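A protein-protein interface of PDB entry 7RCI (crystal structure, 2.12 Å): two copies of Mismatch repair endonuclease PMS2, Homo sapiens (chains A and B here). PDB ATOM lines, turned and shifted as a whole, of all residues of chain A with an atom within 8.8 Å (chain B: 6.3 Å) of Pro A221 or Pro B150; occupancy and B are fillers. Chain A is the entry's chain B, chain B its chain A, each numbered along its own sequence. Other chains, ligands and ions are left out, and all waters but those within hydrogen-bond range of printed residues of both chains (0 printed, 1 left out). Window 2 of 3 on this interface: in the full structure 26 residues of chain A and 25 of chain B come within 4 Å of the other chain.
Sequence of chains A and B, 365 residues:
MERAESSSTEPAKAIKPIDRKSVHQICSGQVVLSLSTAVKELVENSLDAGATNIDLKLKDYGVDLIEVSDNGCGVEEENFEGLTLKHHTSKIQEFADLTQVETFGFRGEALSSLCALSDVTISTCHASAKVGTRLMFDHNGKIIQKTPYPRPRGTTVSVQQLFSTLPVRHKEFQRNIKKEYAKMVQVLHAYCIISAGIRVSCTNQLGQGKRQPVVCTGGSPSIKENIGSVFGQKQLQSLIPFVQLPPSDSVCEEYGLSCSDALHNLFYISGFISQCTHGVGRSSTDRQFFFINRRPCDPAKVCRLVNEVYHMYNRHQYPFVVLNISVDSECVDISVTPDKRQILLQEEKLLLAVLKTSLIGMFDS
Of the 16 printed residues of chain A, 5 touch a printed residue of chain B.
Along chain A the printed residues that touch a printed residue of chain B span positions 197 to 225.
Hydrophobic or aromatic side chains of chain B that line the printed part of chain A: Tyr B149, Pro B150 and Pro B152.
Among the printed residues, no Asp or Glu carboxylate lies within 4 Å of a Lys or Arg side-chain nitrogen of the other chain.
No position is printed for both chains.
Of the 8 pairs that touch across the chains among the printed residues, none has its exchanged pair printed and touching as well.
Among the printed residues, merely in contact across the chains: Gly A197 with Pro B152 (3.4 Å), Gly A219 with Pro B150 (3.9 Å), Gly A219 with Arg B151 (3.7 Å), Gly A219 with Pro B152 (3.2 Å), Pro A221 with Tyr B149 (3.6 Å) and Pro A221 with Pro B150 (3.1 Å).
Printed residues of chain B within 4 Å of Gly A219: Pro B150 (3.9 Å), Arg B151 (3.7 Å) and Pro B152 (3.2 Å).
Printed residues of chain B within 4 Å of Ser A220: Tyr B149 (3.2 Å).
Ser A222 touches none of the printed residues of chain B.
Printed residues of chain A within 4 Å of Tyr B149: Ser A220, Pro A221 and Glu A225.
Of the printed residues of chain A, Pro B150 touches Gly A219 (3.9 Å) and Pro A221 (3.1 Å).
Printed residues of chain A within 4 Å of Arg B151: Gly A219 (3.7 Å).
Printed residues of chain A within 4 Å of Pro B152: Gly A197 and Gly A219.
The nearest residue of chain B that does not touch Pro A221 is Arg B151 (5.3 Å).
The nearest residue of chain A that does not touch Pro B150 is Ser A220 (4.4 Å).
OG of Ser A220 sits close to OE1 of Glu A225, at 3.1 Å.
The backbone carbonyl oxygen of Gly B132 lies within hydrogen-bond range of the backbone NH of Tyr B149, at 2.8 Å.
OG of Ser A222 is in hydrogen-bond range of N of Glu A225, 3.3 Å away.
The backbone NH of Gly A197 sits at hydrogen-bond distance from the backbone carbonyl oxygen of Ser A220, 2.7 Å away.
The side-chain hydroxyl (OH) of Tyr B149 is in hydrogen-bond range of the side-chain carboxylate (OE1) of Glu A225, at 3.4 Å.
OH of Tyr B149 sits at hydrogen-bond distance from OG of Ser A220 (3.2 Å).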
ATOM      1  N   ILE A 193      16.880  20.475 -27.185  1.00  0.00           N
ATOM      2  CA  ILE A 193      17.937  21.389 -26.774  1.00  0.00           C
ATOM      3  C   ILE A 193      17.385  22.458 -25.839  1.00  0.00           C
ATOM      4  O   ILE A 193      18.016  22.809 -24.833  1.00  0.00           O
ATOM      5  CB  ILE A 193      18.608  22.004 -28.017  1.00  0.00           C
ATOM      6  CG1 ILE A 193      19.376  20.933 -28.795  1.00  0.00           C
ATOM      7  CG2 ILE A 193      19.539  23.135 -27.622  1.00  0.00           C
ATOM      8  CD1 ILE A 193      19.829  21.384 -30.172  1.00  0.00           C
ATOM      9  N   ILE A 194      16.195  22.978 -26.141  1.00  0.00           N
ATOM     10  CA  ILE A 194      15.671  24.131 -25.416  1.00  0.00           C
ATOM     11  C   ILE A 194      14.904  23.762 -24.150  1.00  0.00           C
ATOM     12  O   ILE A 194      14.769  24.607 -23.253  1.00  0.00           O
ATOM     13  CB  ILE A 194      14.779  24.980 -26.343  1.00  0.00           C
ATOM     14  CG1 ILE A 194      14.641  26.405 -25.802  1.00  0.00           C
ATOM     15  CG2 ILE A 194      13.413  24.332 -26.520  1.00  0.00           C
ATOM     16  CD1 ILE A 194      15.930  27.194 -25.830  1.00  0.00           C
ATOM     17  N   SER A 195      14.410  22.528 -24.037  1.00  0.00           N
ATOM     18  CA  SER A 195      13.607  22.131 -22.882  1.00  0.00           C
ATOM     19  C   SER A 195      14.539  21.662 -21.770  1.00  0.00           C
ATOM     20  O   SER A 195      14.740  20.469 -21.535  1.00  0.00           O
ATOM     21  CB  SER A 195      12.600  21.056 -23.268  1.00  0.00           C
ATOM     22  OG  SER A 195      11.793  21.490 -24.347  1.00  0.00           O
ATOM     23  N   ALA A 196      15.118  22.635 -21.073  1.00  0.00           N
ATOM     24  CA  ALA A 196      15.971  22.328 -19.937  1.00  0.00           C
ATOM     25  C   ALA A 196      15.126  21.815 -18.781  1.00  0.00           C
ATOM     26  O   ALA A 196      14.031  22.320 -18.519  1.00  0.00           O
ATOM     27  CB  ALA A 196      16.760  23.565 -19.513  1.00  0.00           C
ATOM     28  N   GLY A 197      15.639  20.803 -18.088  1.00  0.00           N
ATOM     29  CA  GLY A 197      14.888  20.197 -17.010  1.00  0.00           C
ATOM     30  C   GLY A 197      13.749  19.319 -17.465  1.00  0.00           C
ATOM     31  O   GLY A 197      12.921  18.924 -16.640  1.00  0.00           O
ATOM     32  N   ILE A 198      13.679  19.005 -18.757  1.00  0.00           N
ATOM     33  CA  ILE A 198      12.628  18.169 -19.320  1.00  0.00           C
ATOM     34  C   ILE A 198      13.289  17.029 -20.075  1.00  0.00           C
ATOM     35  O   ILE A 198      14.162  17.261 -20.919  1.00  0.00           O
ATOM     36  CB  ILE A 198      11.700  18.967 -20.258  1.00  0.00           C
ATOM     37  CG1 ILE A 198      11.115  20.173 -19.527  1.00  0.00           C
ATOM     38  CG2 ILE A 198      10.587  18.075 -20.791  1.00  0.00           C
ATOM     39  CD1 ILE A 198      10.170  20.996 -20.360  1.00  0.00           C
ATOM     40  N   GLY A 218      18.526  13.835 -20.673  1.00  0.00           N
ATOM     41  CA  GLY A 218      18.517  13.431 -19.284  1.00  0.00           C
ATOM     42  C   GLY A 218      17.806  14.365 -18.330  1.00  0.00           C
ATOM     43  O   GLY A 218      17.898  14.165 -17.113  1.00  0.00           O
ATOM     44  N   GLY A 219      17.104  15.377 -18.830  1.00  0.00           N
ATOM     45  CA  GLY A 219      16.476  16.341 -17.951  1.00  0.00           C
ATOM     46  C   GLY A 219      17.439  17.334 -17.350  1.00  0.00           C
ATOM     47  O   GLY A 219      17.230  17.787 -16.221  1.00  0.00           O
ATOM     48  N   SER A 220      18.495  17.681 -18.070  1.00  0.00           N
ATOM     49  CA  SER A 220      19.521  18.568 -17.553  1.00  0.00           C
ATOM     50  C   SER A 220      19.039  20.018 -17.571  1.00  0.00           C
ATOM     51  O   SER A 220      18.292  20.422 -18.465  1.00  0.00           O
ATOM     52  CB  SER A 220      20.795  18.435 -18.378  1.00  0.00           C
ATOM     53  OG  SER A 220      21.871  19.135 -17.780  1.00  0.00           O
ATOM     54  N   PRO A 221      19.454  20.821 -16.585  1.00  0.00           N
ATOM     55  CA  PRO A 221      19.009  22.221 -16.532  1.00  0.00           C
ATOM     56  C   PRO A 221      19.728  23.142 -17.500  1.00  0.00           C
ATOM     57  O   PRO A 221      19.325  24.306 -17.632  1.00  0.00           O
ATOM     58  CB  PRO A 221      19.307  22.620 -15.082  1.00  0.00           C
ATOM     59  CG  PRO A 221      20.479  21.776 -14.710  1.00  0.00           C
ATOM     60  CD  PRO A 221      20.288  20.462 -15.423  1.00  0.00           C
ATOM     61  N   SER A 222      20.769  22.670 -18.179  1.00  0.00           N
ATOM     62  CA  SER A 222      21.564  23.507 -19.062  1.00  0.00           C
ATOM     63  C   SER A 222      21.345  23.118 -20.518  1.00  0.00           C
ATOM     64  O   SER A 222      21.078  21.957 -20.840  1.00  0.00           O
ATOM     65  CB  SER A 222      23.053  23.404 -18.714  1.00  0.00           C
ATOM     66  OG  SER A 222      23.599  22.175 -19.160  1.00  0.00           O
ATOM     67  N   ILE A 223      21.464  24.115 -21.396  1.00  0.00           N
ATOM     68  CA  ILE A 223      21.340  23.874 -22.827  1.00  0.00           C
ATOM     69  C   ILE A 223      22.558  23.127 -23.350  1.00  0.00           C
ATOM     70  O   ILE A 223      22.446  22.310 -24.273  1.00  0.00           O
ATOM     71  CB  ILE A 223      21.123  25.212 -23.562  1.00  0.00           C
ATOM     72  CG1 ILE A 223      19.771  25.811 -23.172  1.00  0.00           C
ATOM     73  CG2 ILE A 223      21.214  25.032 -25.067  1.00  0.00           C
ATOM     74  CD1 ILE A 223      19.454  27.108 -23.872  1.00  0.00           C
ATOM     75  N   LYS A 224      23.732  23.378 -22.766  1.00  0.00           N
ATOM     76  CA  LYS A 224      24.949  22.720 -23.229  1.00  0.00           C
ATOM     77  C   LYS A 224      24.856  21.202 -23.099  1.00  0.00           C
ATOM     78  O   LYS A 224      25.240  20.471 -24.021  1.00  0.00           O
ATOM     79  CB  LYS A 224      26.152  23.257 -22.454  1.00  0.00           C
ATOM     80  CG  LYS A 224      27.496  22.746 -22.945  1.00  0.00           C
ATOM     81  CD  LYS A 224      28.606  23.149 -21.989  1.00  0.00           C
ATOM     82  CE  LYS A 224      29.540  24.173 -22.609  1.00  0.00           C
ATOM     83  NZ  LYS A 224      30.759  23.540 -23.185  1.00  0.00           N
ATOM     84  N   GLU A 225      24.345  20.704 -21.967  1.00  0.00           N
ATOM     85  CA  GLU A 225      24.211  19.257 -21.811  1.00  0.00           C
ATOM     86  C   GLU A 225      23.160  18.681 -22.750  1.00  0.00           C
ATOM     87  O   GLU A 225      23.306  17.547 -23.217  1.00  0.00           O
ATOM     88  CB  GLU A 225      23.885  18.882 -20.362  1.00  0.00           C
ATOM     89  CG  GLU A 225      25.105  18.808 -19.447  1.00  0.00           C
ATOM     90  CD  GLU A 225      24.771  18.328 -18.040  1.00  0.00           C
ATOM     91  OE1 GLU A 225      24.309  17.175 -17.900  1.00  0.00           O
ATOM     92  OE2 GLU A 225      24.971  19.098 -17.075  1.00  0.00           O
ATOM     93  N   ASN A 226      22.097  19.437 -23.033  1.00  0.00           N
ATOM     94  CA  ASN A 226      21.100  18.961 -23.984  1.00  0.00           C
ATOM     95  C   ASN A 226      21.699  18.831 -25.378  1.00  0.00           C
ATOM     96  O   ASN A 226      21.345  17.916 -26.130  1.00  0.00           O
ATOM     97  CB  ASN A 226      19.896  19.902 -23.996  1.00  0.00           C
ATOM     98  CG  ASN A 226      19.020  19.740 -22.770  1.00  0.00           C
ATOM     99  OD1 ASN A 226      19.105  18.738 -22.059  1.00  0.00           O
ATOM    100  ND2 ASN A 226      18.175  20.731 -22.512  1.00  0.00           N
ATOM    101  N   ARG A 294      12.570  31.147 -26.404  1.00  0.00           N
ATOM    102  CA  ARG A 294      12.714  29.699 -26.273  1.00  0.00           C
ATOM    103  C   ARG A 294      11.730  28.926 -27.140  1.00  0.00           C
ATOM    104  O   ARG A 294      11.406  27.774 -26.840  1.00  0.00           O
ATOM    105  CB  ARG A 294      12.598  29.263 -24.811  1.00  0.00           C
ATOM    106  CG  ARG A 294      13.367  30.159 -23.867  1.00  0.00           C
ATOM    107  CD  ARG A 294      13.417  29.567 -22.491  1.00  0.00           C
ATOM    108  NE  ARG A 294      14.227  28.356 -22.445  1.00  0.00           N
ATOM    109  CZ  ARG A 294      15.531  28.337 -22.204  1.00  0.00           C
ATOM    110  NH1 ARG A 294      16.209  29.452 -21.984  1.00  0.00           N
ATOM    111  NH2 ARG A 294      16.170  27.171 -22.182  1.00  0.00           N
ATOM    112  N   VAL B 131      14.390  21.632  -5.143  1.00  0.00           N
ATOM    113  CA  VAL B 131      15.415  21.577  -6.178  1.00  0.00           C
ATOM    114  C   VAL B 131      16.195  20.279  -6.019  1.00  0.00           C
ATOM    115  O   VAL B 131      16.379  19.774  -4.908  1.00  0.00           O
ATOM    116  CB  VAL B 131      16.369  22.797  -6.107  1.00  0.00           C
ATOM    117  CG1 VAL B 131      17.394  22.764  -7.234  1.00  0.00           C
ATOM    118  CG2 VAL B 131      15.585  24.100  -6.139  1.00  0.00           C
ATOM    119  N   GLY B 132      16.647  19.731  -7.146  1.00  0.00           N
ATOM    120  CA  GLY B 132      17.470  18.545  -7.132  1.00  0.00           C
ATOM    121  C   GLY B 132      18.895  18.844  -6.704  1.00  0.00           C
ATOM    122  O   GLY B 132      19.262  19.971  -6.374  1.00  0.00           O
ATOM    123  N   THR B 133      19.717  17.800  -6.722  1.00  0.00           N
ATOM    124  CA  THR B 133      21.097  17.904  -6.274  1.00  0.00           C
ATOM    125  C   THR B 133      21.980  17.015  -7.136  1.00  0.00           C
ATOM    126  O   THR B 133      21.525  16.006  -7.679  1.00  0.00           O
ATOM    127  CB  THR B 133      21.240  17.506  -4.797  1.00  0.00           C
ATOM    128  OG1 THR B 133      20.110  17.988  -4.059  1.00  0.00           O
ATOM    129  CG2 THR B 133      22.508  18.102  -4.202  1.00  0.00           C
ATOM    130  N   PRO B 148      23.315  22.137  -5.850  1.00  0.00           N
ATOM    131  CA  PRO B 148      21.935  22.088  -6.342  1.00  0.00           C
ATOM    132  C   PRO B 148      21.901  21.879  -7.848  1.00  0.00           C
ATOM    133  O   PRO B 148      22.663  22.489  -8.599  1.00  0.00           O
ATOM    134  CB  PRO B 148      21.367  23.453  -5.944  1.00  0.00           C
ATOM    135  CG  PRO B 148      22.205  23.885  -4.789  1.00  0.00           C
ATOM    136  CD  PRO B 148      23.581  23.357  -5.069  1.00  0.00           C
ATOM    137  N   TYR B 149      21.000  21.000  -8.283  1.00  0.00           N
ATOM    138  CA  TYR B 149      20.932  20.576  -9.678  1.00  0.00           C
ATOM    139  C   TYR B 149      19.467  20.536 -10.093  1.00  0.00           C
ATOM    140  O   TYR B 149      18.739  19.595  -9.735  1.00  0.00           O
ATOM    141  CB  TYR B 149      21.597  19.213  -9.847  1.00  0.00           C
ATOM    142  CG  TYR B 149      21.793  18.751 -11.270  1.00  0.00           C
ATOM    143  CD1 TYR B 149      22.831  19.252 -12.046  1.00  0.00           C
ATOM    144  CD2 TYR B 149      20.963  17.786 -11.826  1.00  0.00           C
ATOM    145  CE1 TYR B 149      23.022  18.821 -13.343  1.00  0.00           C
ATOM    146  CE2 TYR B 149      21.147  17.349 -13.122  1.00  0.00           C
ATOM    147  CZ  TYR B 149      22.178  17.869 -13.876  1.00  0.00           C
ATOM    148  OH  TYR B 149      22.366  17.437 -15.169  1.00  0.00           O
ATOM    149  N   PRO B 150      19.000  21.525 -10.854  1.00  0.00           N
ATOM    150  CA  PRO B 150      17.590  21.529 -11.267  1.00  0.00           C
ATOM    151  C   PRO B 150      17.305  20.429 -12.273  1.00  0.00           C
ATOM    152  O   PRO B 150      17.802  20.463 -13.402  1.00  0.00           O
ATOM    153  CB  PRO B 150      17.402  22.923 -11.881  1.00  0.00           C
ATOM    154  CG  PRO B 150      18.540  23.743 -11.341  1.00  0.00           C
ATOM    155  CD  PRO B 150      19.680  22.783 -11.200  1.00  0.00           C
ATOM    156  N   ARG B 151      16.498  19.453 -11.880  1.00  0.00           N
ATOM    157  CA  ARG B 151      16.235  18.292 -12.714  1.00  0.00           C
ATOM    158  C   ARG B 151      14.867  17.743 -12.355  1.00  0.00           C
ATOM    159  O   ARG B 151      14.369  17.985 -11.248  1.00  0.00           O
ATOM    160  CB  ARG B 151      17.311  17.212 -12.522  1.00  0.00           C
ATOM    161  CG  ARG B 151      17.531  16.819 -11.070  1.00  0.00           C
ATOM    162  CD  ARG B 151      18.040  15.402 -10.962  1.00  0.00           C
ATOM    163  NE  ARG B 151      17.020  14.456 -11.393  1.00  0.00           N
ATOM    164  CZ  ARG B 151      17.234  13.467 -12.247  1.00  0.00           C
ATOM    165  NH1 ARG B 151      18.428  13.260 -12.777  1.00  0.00           N
ATOM    166  NH2 ARG B 151      16.223  12.673 -12.585  1.00  0.00           N
ATOM    167  N   PRO B 152      14.230  17.006 -13.263  1.00  0.00           N
ATOM    168  CA  PRO B 152      12.956  16.366 -12.924  1.00  0.00           C
ATOM    169  C   PRO B 152      13.147  15.324 -11.832  1.00  0.00           C
ATOM    170  O   PRO B 152      14.262  14.887 -11.537  1.00  0.00           O
ATOM    171  CB  PRO B 152      12.515  15.720 -14.246  1.00  0.00           C
ATOM    172  CG  PRO B 152      13.768  15.579 -15.039  1.00  0.00           C
ATOM    173  CD  PRO B 152      14.623  16.748 -14.659  1.00  0.00           C
